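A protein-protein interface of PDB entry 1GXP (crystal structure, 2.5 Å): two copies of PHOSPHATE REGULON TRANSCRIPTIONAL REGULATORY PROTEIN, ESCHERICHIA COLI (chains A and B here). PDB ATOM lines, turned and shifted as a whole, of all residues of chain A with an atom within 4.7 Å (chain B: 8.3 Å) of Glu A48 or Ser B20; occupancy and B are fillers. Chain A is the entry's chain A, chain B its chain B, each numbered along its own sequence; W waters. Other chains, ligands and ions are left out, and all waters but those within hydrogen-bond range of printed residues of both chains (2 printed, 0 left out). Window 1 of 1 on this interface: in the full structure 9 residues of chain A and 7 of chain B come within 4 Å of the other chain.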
ATOM      1  N   HIS A  46      23.916  -1.993 -12.800  1.00  0.00           N
ATOM      2  CA  HIS A  46      22.470  -1.835 -12.668  1.00  0.00           C
ATOM      3  C   HIS A  46      21.780  -3.175 -12.855  1.00  0.00           C
ATOM      4  O   HIS A  46      21.043  -3.392 -13.816  1.00  0.00           O
ATOM      5  CB  HIS A  46      21.965  -0.826 -13.699  1.00  0.00           C
ATOM      6  CG  HIS A  46      22.713   0.467 -13.661  1.00  0.00           C
ATOM      7  ND1 HIS A  46      23.966   0.611 -14.219  1.00  0.00           N
ATOM      8  CD2 HIS A  46      22.437   1.636 -13.037  1.00  0.00           C
ATOM      9  CE1 HIS A  46      24.430   1.814 -13.933  1.00  0.00           C
ATOM     10  NE2 HIS A  46      23.525   2.457 -13.216  1.00  0.00           N
ATOM     11  N   PRO A  47      22.025  -4.100 -11.931  1.00  0.00           N
ATOM     12  CA  PRO A  47      21.436  -5.441 -11.979  1.00  0.00           C
ATOM     13  C   PRO A  47      20.027  -5.522 -11.382  1.00  0.00           C
ATOM     14  O   PRO A  47      19.552  -4.575 -10.746  1.00  0.00           O
ATOM     15  CB  PRO A  47      22.438  -6.262 -11.183  1.00  0.00           C
ATOM     16  CG  PRO A  47      22.831  -5.287 -10.094  1.00  0.00           C
ATOM     17  CD  PRO A  47      23.019  -3.994 -10.847  1.00  0.00           C
ATOM     18  N   GLU A  48      19.366  -6.657 -11.595  1.00  0.00           N
ATOM     19  CA  GLU A  48      18.031  -6.889 -11.052  1.00  0.00           C
ATOM     20  C   GLU A  48      17.152  -5.671 -11.306  1.00  0.00           C
ATOM     21  O   GLU A  48      16.406  -5.224 -10.431  1.00  0.00           O
ATOM     22  CB  GLU A  48      18.117  -7.152  -9.543  1.00  0.00           C
ATOM     23  CG  GLU A  48      19.252  -8.085  -9.097  1.00  0.00           C
ATOM     24  CD  GLU A  48      19.344  -9.383  -9.915  1.00  0.00           C
ATOM     25  OE1 GLU A  48      18.309  -9.812 -10.475  1.00  0.00           O
ATOM     26  OE2 GLU A  48      20.453  -9.976  -9.989  1.00  0.00           O
ATOM     27  N   ARG A  49      17.253  -5.134 -12.516  1.00  0.00           N
ATOM     28  CA  ARG A  49      16.487  -3.961 -12.899  1.00  0.00           C
ATOM     29  C   ARG A  49      16.340  -3.999 -14.403  1.00  0.00           C
ATOM     30  O   ARG A  49      17.320  -3.892 -15.114  1.00  0.00           O
ATOM     31  CB  ARG A  49      17.236  -2.709 -12.465  1.00  0.00           C
ATOM     32  CG  ARG A  49      16.476  -1.456 -12.722  1.00  0.00           C
ATOM     33  CD  ARG A  49      17.249  -0.235 -12.279  1.00  0.00           C
ATOM     34  NE  ARG A  49      16.545   0.984 -12.661  1.00  0.00           N
ATOM     35  CZ  ARG A  49      17.025   2.209 -12.479  1.00  0.00           C
ATOM     36  NH1 ARG A  49      18.222   2.371 -11.914  1.00  0.00           N
ATOM     37  NH2 ARG A  49      16.308   3.270 -12.854  1.00  0.00           N
ATOM     38  N   VAL A  50      15.118  -4.168 -14.887  1.00  0.00           N
ATOM     39  CA  VAL A  50      14.875  -4.248 -16.328  1.00  0.00           C
ATOM     40  C   VAL A  50      14.981  -2.900 -17.055  1.00  0.00           C
ATOM     41  O   VAL A  50      14.559  -1.854 -16.556  1.00  0.00           O
ATOM     42  CB  VAL A  50      13.488  -4.855 -16.624  1.00  0.00           C
ATOM     43  CG1 VAL A  50      12.402  -3.866 -16.228  1.00  0.00           C
ATOM     44  CG2 VAL A  50      13.376  -5.219 -18.099  1.00  0.00           C
ATOM     45  N   ARG A 101      17.298  -7.509 -18.861  1.00  0.00           N
ATOM     46  CA  ARG A 101      17.700  -7.317 -17.478  1.00  0.00           C
ATOM     47  C   ARG A 101      18.939  -8.124 -17.122  1.00  0.00           C
ATOM     48  O   ARG A 101      19.182  -9.197 -17.689  1.00  0.00           O
ATOM     49  CB  ARG A 101      16.544  -7.738 -16.565  1.00  0.00           C
ATOM     50  CG  ARG A 101      16.977  -8.317 -15.217  1.00  0.00           C
ATOM     51  CD  ARG A 101      15.764  -8.864 -14.488  1.00  0.00           C
ATOM     52  NE  ARG A 101      15.166  -9.978 -15.209  1.00  0.00           N
ATOM     53  CZ  ARG A 101      13.884 -10.314 -15.141  1.00  0.00           C
ATOM     54  NH1 ARG A 101      13.050  -9.614 -14.386  1.00  0.00           N
ATOM     55  NH2 ARG A 101      13.438 -11.365 -15.817  1.00  0.00           N
ATOM     56  N   PHE A 102      19.723  -7.626 -16.180  1.00  0.00           N
ATOM     57  CA  PHE A 102      20.892  -8.384 -15.798  1.00  0.00           C
ATOM     58  C   PHE A 102      20.629  -8.863 -14.389  1.00  0.00           C
ATOM     59  O   PHE A 102      20.364  -8.055 -13.481  1.00  0.00           O
ATOM     60  CB  PHE A 102      22.163  -7.549 -15.858  1.00  0.00           C
ATOM     61  CG  PHE A 102      23.405  -8.371 -15.713  1.00  0.00           C
ATOM     62  CD1 PHE A 102      24.083  -8.433 -14.495  1.00  0.00           C
ATOM     63  CD2 PHE A 102      23.861  -9.162 -16.771  1.00  0.00           C
ATOM     64  CE1 PHE A 102      25.195  -9.283 -14.336  1.00  0.00           C
ATOM     65  CE2 PHE A 102      24.966 -10.009 -16.615  1.00  0.00           C
ATOM     66  CZ  PHE A 102      25.627 -10.064 -15.395  1.00  0.00           C
ATOM     67  N   SER A 103      20.686 -10.180 -14.211  1.00  0.00           N
ATOM     68  CA  SER A 103      20.405 -10.763 -12.912  1.00  0.00           C
ATOM     69  C   SER A 103      21.244 -11.995 -12.585  1.00  0.00           C
ATOM     70  O   SER A 103      21.715 -12.703 -13.477  1.00  0.00           O
ATOM     71  CB  SER A 103      18.913 -11.123 -12.842  1.00  0.00           C
ATOM     72  OG  SER A 103      18.616 -11.920 -11.707  1.00  0.00           O
ATOM     73  N   THR A 104      21.426 -12.225 -11.290  1.00  0.00           N
ATOM     74  CA  THR A 104      22.173 -13.369 -10.800  1.00  0.00           C
ATOM     75  C   THR A 104      21.168 -14.454 -10.379  1.00  0.00           C
ATOM     76  O   THR A 104      21.488 -15.651 -10.352  1.00  0.00           O
ATOM     77  CB  THR A 104      23.029 -12.993  -9.578  1.00  0.00           C
ATOM     78  OG1 THR A 104      22.210 -12.316  -8.617  1.00  0.00           O
ATOM     79  CG2 THR A 104      24.190 -12.097  -9.994  1.00  0.00           C
ATOM     80  N   ARG A 105      19.951 -14.028 -10.057  1.00  0.00           N
ATOM     81  CA  ARG A 105      18.924 -14.964  -9.647  1.00  0.00           C
ATOM     82  C   ARG A 105      18.266 -15.551 -10.874  1.00  0.00           C
ATOM     83  O   ARG A 105      17.581 -14.856 -11.604  1.00  0.00           O
ATOM     84  CB  ARG A 105      17.890 -14.261  -8.762  1.00  0.00           C
ATOM     85  CG  ARG A 105      18.512 -13.726  -7.494  1.00  0.00           C
ATOM     86  CD  ARG A 105      17.485 -13.336  -6.458  1.00  0.00           C
ATOM     87  NE  ARG A 105      16.739 -12.140  -6.833  1.00  0.00           N
ATOM     88  CZ  ARG A 105      17.291 -10.951  -7.060  1.00  0.00           C
ATOM     89  NH1 ARG A 105      16.518  -9.923  -7.394  1.00  0.00           N
ATOM     90  NH2 ARG A 105      18.609 -10.792  -6.960  1.00  0.00           N
ATOM     91  N   VAL B   8       9.031  -3.225  -3.798  1.00  0.00           N
ATOM     92  CA  VAL B   8       8.921  -4.671  -3.873  1.00  0.00           C
ATOM     93  C   VAL B   8       7.838  -5.119  -2.903  1.00  0.00           C
ATOM     94  O   VAL B   8       7.848  -4.751  -1.727  1.00  0.00           O
ATOM     95  CB  VAL B   8      10.241  -5.371  -3.481  1.00  0.00           C
ATOM     96  CG1 VAL B   8      10.043  -6.876  -3.466  1.00  0.00           C
ATOM     97  CG2 VAL B   8      11.338  -5.003  -4.457  1.00  0.00           C
ATOM     98  N   SER B  15       7.245 -12.705  -3.753  1.00  0.00           N
ATOM     99  CA  SER B  15       7.620 -11.323  -3.991  1.00  0.00           C
ATOM    100  C   SER B  15       7.408 -10.877  -5.425  1.00  0.00           C
ATOM    101  O   SER B  15       7.530 -11.669  -6.366  1.00  0.00           O
ATOM    102  CB  SER B  15       9.088 -11.125  -3.616  1.00  0.00           C
ATOM    103  OG  SER B  15       9.913 -11.987  -4.393  1.00  0.00           O
ATOM    104  N   LEU B  16       7.067  -9.604  -5.583  1.00  0.00           N
ATOM    105  CA  LEU B  16       6.888  -9.035  -6.910  1.00  0.00           C
ATOM    106  C   LEU B  16       7.551  -7.665  -6.891  1.00  0.00           C
ATOM    107  O   LEU B  16       7.110  -6.766  -6.185  1.00  0.00           O
ATOM    108  CB  LEU B  16       5.402  -8.928  -7.282  1.00  0.00           C
ATOM    109  CG  LEU B  16       5.157  -8.435  -8.714  1.00  0.00           C
ATOM    110  CD1 LEU B  16       3.795  -8.884  -9.200  1.00  0.00           C
ATOM    111  CD2 LEU B  16       5.305  -6.917  -8.771  1.00  0.00           C
ATOM    112  N   ASP B  17       8.646  -7.541  -7.638  1.00  0.00           N
ATOM    113  CA  ASP B  17       9.410  -6.291  -7.738  1.00  0.00           C
ATOM    114  C   ASP B  17       9.197  -5.684  -9.121  1.00  0.00           C
ATOM    115  O   ASP B  17       9.634  -6.231 -10.136  1.00  0.00           O
ATOM    116  CB  ASP B  17      10.907  -6.547  -7.500  1.00  0.00           C
ATOM    117  CG  ASP B  17      11.777  -5.336  -7.833  1.00  0.00           C
ATOM    118  OD1 ASP B  17      12.781  -5.093  -7.110  1.00  0.00           O
ATOM    119  OD2 ASP B  17      11.464  -4.637  -8.828  1.00  0.00           O
ATOM    120  N   PRO B  18       8.522  -4.534  -9.167  1.00  0.00           N
ATOM    121  CA  PRO B  18       8.206  -3.796 -10.394  1.00  0.00           C
ATOM    122  C   PRO B  18       9.482  -3.439 -11.147  1.00  0.00           C
ATOM    123  O   PRO B  18       9.616  -3.724 -12.348  1.00  0.00           O
ATOM    124  CB  PRO B  18       7.468  -2.562  -9.875  1.00  0.00           C
ATOM    125  CG  PRO B  18       6.912  -3.019  -8.534  1.00  0.00           C
ATOM    126  CD  PRO B  18       8.079  -3.793  -7.978  1.00  0.00           C
ATOM    127  N   THR B  19      10.411  -2.818 -10.422  1.00  0.00           N
ATOM    128  CA  THR B  19      11.705  -2.429 -10.969  1.00  0.00           C
ATOM    129  C   THR B  19      12.241  -3.570 -11.836  1.00  0.00           C
ATOM    130  O   THR B  19      12.267  -3.477 -13.061  1.00  0.00           O
ATOM    131  CB  THR B  19      12.720  -2.151  -9.841  1.00  0.00           C
ATOM    132  OG1 THR B  19      12.104  -1.339  -8.837  1.00  0.00           O
ATOM    133  CG2 THR B  19      13.924  -1.417 -10.369  1.00  0.00           C
ATOM    134  N   SER B  20      12.662  -4.656 -11.206  1.00  0.00           N
ATOM    135  CA  SER B  20      13.186  -5.795 -11.952  1.00  0.00           C
ATOM    136  C   SER B  20      12.107  -6.484 -12.788  1.00  0.00           C
ATOM    137  O   SER B  20      12.404  -7.249 -13.698  1.00  0.00           O
ATOM    138  CB  SER B  20      13.801  -6.797 -10.983  1.00  0.00           C
ATOM    139  OG  SER B  20      12.932  -6.983  -9.868  1.00  0.00           O
ATOM    140  N   HIS B  21      10.847  -6.192 -12.484  1.00  0.00           N
ATOM    141  CA  HIS B  21       9.728  -6.815 -13.190  1.00  0.00           C
ATOM    142  C   HIS B  21       9.893  -8.322 -13.009  1.00  0.00           C
ATOM    143  O   HIS B  21      10.044  -9.060 -13.979  1.00  0.00           O
ATOM    144  CB  HIS B  21       9.750  -6.446 -14.687  1.00  0.00           C
ATOM    145  CG  HIS B  21       8.466  -6.742 -15.404  1.00  0.00           C
ATOM    146  ND1 HIS B  21       8.161  -7.984 -15.915  1.00  0.00           N
ATOM    147  CD2 HIS B  21       7.376  -5.969 -15.631  1.00  0.00           C
ATOM    148  CE1 HIS B  21       6.940  -7.969 -16.422  1.00  0.00           C
ATOM    149  NE2 HIS B  21       6.443  -6.756 -16.261  1.00  0.00           N
ATOM    150  N   ARG B  22       9.869  -8.771 -11.757  1.00  0.00           N
ATOM    151  CA  ARG B  22      10.043 -10.189 -11.474  1.00  0.00           C
ATOM    152  C   ARG B  22       9.232 -10.814 -10.331  1.00  0.00           C
ATOM    153  O   ARG B  22       8.968 -10.185  -9.293  1.00  0.00           O
ATOM    154  CB  ARG B  22      11.515 -10.461 -11.228  1.00  0.00           C
ATOM    155  CG  ARG B  22      11.912 -11.849 -11.632  1.00  0.00           C
ATOM    156  CD  ARG B  22      13.373 -11.880 -11.862  1.00  0.00           C
ATOM    157  NE  ARG B  22      13.764 -13.034 -12.637  1.00  0.00           N
ATOM    158  CZ  ARG B  22      15.015 -13.454 -12.710  1.00  0.00           C
ATOM    159  NH1 ARG B  22      15.959 -12.795 -12.054  1.00  0.00           N
ATOM    160  NH2 ARG B  22      15.317 -14.535 -13.414  1.00  0.00           N
ATOM    161  N   VAL B  23       8.860 -12.071 -10.523  1.00  0.00           N
ATOM    162  CA  VAL B  23       8.097 -12.776  -9.502  1.00  0.00           C
ATOM    163  C   VAL B  23       8.899 -13.949  -8.972  1.00  0.00           C
ATOM    164  O   VAL B  23       9.270 -14.867  -9.721  1.00  0.00           O
ATOM    165  CB  VAL B  23       6.724 -13.282 -10.062  1.00  0.00           C
ATOM    166  CG1 VAL B  23       6.158 -14.406  -9.181  1.00  0.00           C
ATOM    167  CG2 VAL B  23       5.721 -12.111 -10.122  1.00  0.00           C
ATOM    168  N   MET B  24       9.163 -13.920  -7.672  1.00  0.00           N
ATOM    169  CA  MET B  24       9.928 -14.996  -7.051  1.00  0.00           C
ATOM    170  C   MET B  24       9.337 -15.660  -5.818  1.00  0.00           C
ATOM    171  O   MET B  24       8.996 -14.994  -4.830  1.00  0.00           O
ATOM    172  CB  MET B  24      11.337 -14.525  -6.675  1.00  0.00           C
ATOM    173  CG  MET B  24      12.280 -14.318  -7.848  1.00  0.00           C
ATOM    174  SD  MET B  24      13.980 -14.149  -7.301  1.00  0.00           S
ATOM    175  CE  MET B  24      13.852 -12.767  -6.136  1.00  0.00           C
ATOM    176  N   GLU B  27      13.763 -17.754  -3.305  1.00  0.00           N
ATOM    177  CA  GLU B  27      14.808 -17.354  -4.243  1.00  0.00           C
ATOM    178  C   GLU B  27      14.482 -17.878  -5.650  1.00  0.00           C
ATOM    179  O   GLU B  27      15.164 -17.548  -6.628  1.00  0.00           O
ATOM    180  CB  GLU B  27      16.170 -17.890  -3.760  1.00  0.00           C
ATOM    181  CG  GLU B  27      17.382 -17.602  -4.670  1.00  0.00           C
ATOM    182  CD  GLU B  27      17.725 -16.112  -4.821  1.00  0.00           C
ATOM    183  OE1 GLU B  27      18.715 -15.810  -5.531  1.00  0.00           O
ATOM    184  OE2 GLU B  27      17.019 -15.252  -4.244  1.00  0.00           O
ATOM    185  N   PHE B  37       1.370 -11.209 -14.861  1.00  0.00           N
ATOM    186  CA  PHE B  37       2.169 -10.348 -14.016  1.00  0.00           C
ATOM    187  C   PHE B  37       1.300  -9.182 -13.551  1.00  0.00           C
ATOM    188  O   PHE B  37       1.285  -8.826 -12.367  1.00  0.00           O
ATOM    189  CB  PHE B  37       3.377  -9.821 -14.777  1.00  0.00           C
ATOM    190  CG  PHE B  37       4.328  -9.059 -13.916  1.00  0.00           C
ATOM    191  CD1 PHE B  37       5.334  -9.724 -13.211  1.00  0.00           C
ATOM    192  CD2 PHE B  37       4.180  -7.686 -13.753  1.00  0.00           C
ATOM    193  CE1 PHE B  37       6.181  -9.016 -12.346  1.00  0.00           C
ATOM    194  CE2 PHE B  37       5.016  -6.976 -12.897  1.00  0.00           C
ATOM    195  CZ  PHE B  37       6.014  -7.631 -12.192  1.00  0.00           C
HETATM  196  O   HOH W   1      15.501 -10.487 -10.387  1.00  0.00           O
HETATM  197  O   HOH W   2      13.924  -9.210  -7.710  1.00  0.00           O
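Of the 10 printed residues of chain A, 6 touch a printed residue of chain B. Along chain A the printed residues that touch a printed residue of chain B span positions 48 to 105. Hydrophobic or aromatic side chains of chain B that line the printed part of chain A: Met B24. Along chain B the printed residues that touch a printed residue of chain A span positions 19 to 27. Among the printed residues, 12 pairs touch across the chains.
No position is printed for both chains.
OE2 of Glu A48 is in hydrogen-bond range of N of Thr A104, at 2.8 Å. The backbone carbonyl oxygen (O) of Ser B15 sits at hydrogen-bond distance from the backbone NH (N) of Met B24. OG of Ser A103 is in hydrogen-bond range of N of Arg A105 (3.0 Å). N of Ser B20 is in hydrogen-bond range of OD2 of Asp B17 (2.7 Å). The backbone NH of Glu A48 lies within hydrogen-bond range of the backbone carbonyl oxygen of Phe A102, 2.6 Å away. The side-chain carboxylate of Glu A48 is in salt-bridge range of the guanidinium group of Arg A105.
Glu A48 touches just one residue of chain B: Ser B20 (3.1 Å). Of the printed residues of chain A, Arg B22 touches Arg A101 (3.4 Å), Ser A103 (2.8 Å) and Arg A105 (2.7 Å). Of the printed residues of chain A, Glu B27 touches Arg A105 (2.9 Å). Of the printed residues of chain B, Arg A101 touches Ser B20 (2.5 Å), His B21 (3.1 Å) and Arg B22 (3.4 Å). Printed residues of chain B within 4 Å of Val A50: Thr B19 (3.2 Å) and Ser B20 (3.9 Å). His A46 touches none of the printed residues of chain B. Phe A102 touches none of the printed residues of chain B. The nearest printed residue of chain A that does not touch Ser B20 is Arg A105 (5.3 Å).
Among the printed residues, pairs that only touch across the chains: Arg A105 with Glu B27, Glu A48 with Ser B20, Arg A101 with Arg B22, Arg A49 with Thr B19, Val A50 with Ser B20 and Arg A49 with Ser B20.
Water W2 bridges the guanidinium group (NH1) of Arg A105 (2.7 Å) and the side-chain hydroxyl (OG) of Ser B20 (3.3 Å). Water W1 lies within hydrogen-bond range of the guanidinium group of Arg B22, the side-chain carboxylate of Glu A48 and the guanidinium group of Arg A105.
OG of Ser A103 lies within hydrogen-bond range of NH1 of Arg B22, at 2.8 Å. The guanidinium group (NH1) of Arg A101 is in hydrogen-bond range of the backbone carbonyl oxygen (O) of Ser B20, 2.5 Å away. NH1 of Arg B22 sits at hydrogen-bond distance from O of Arg A105 (2.7 Å). NE of Arg A105 lies close to SD of Met B24. The backbone carbonyl oxygen (O) of His B21 lies within hydrogen-bond range of the guanidinium group (NH1) of Arg A101 (3.1 Å). N of Val A50 lies close to O of Thr B19, at 3.5 Å.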
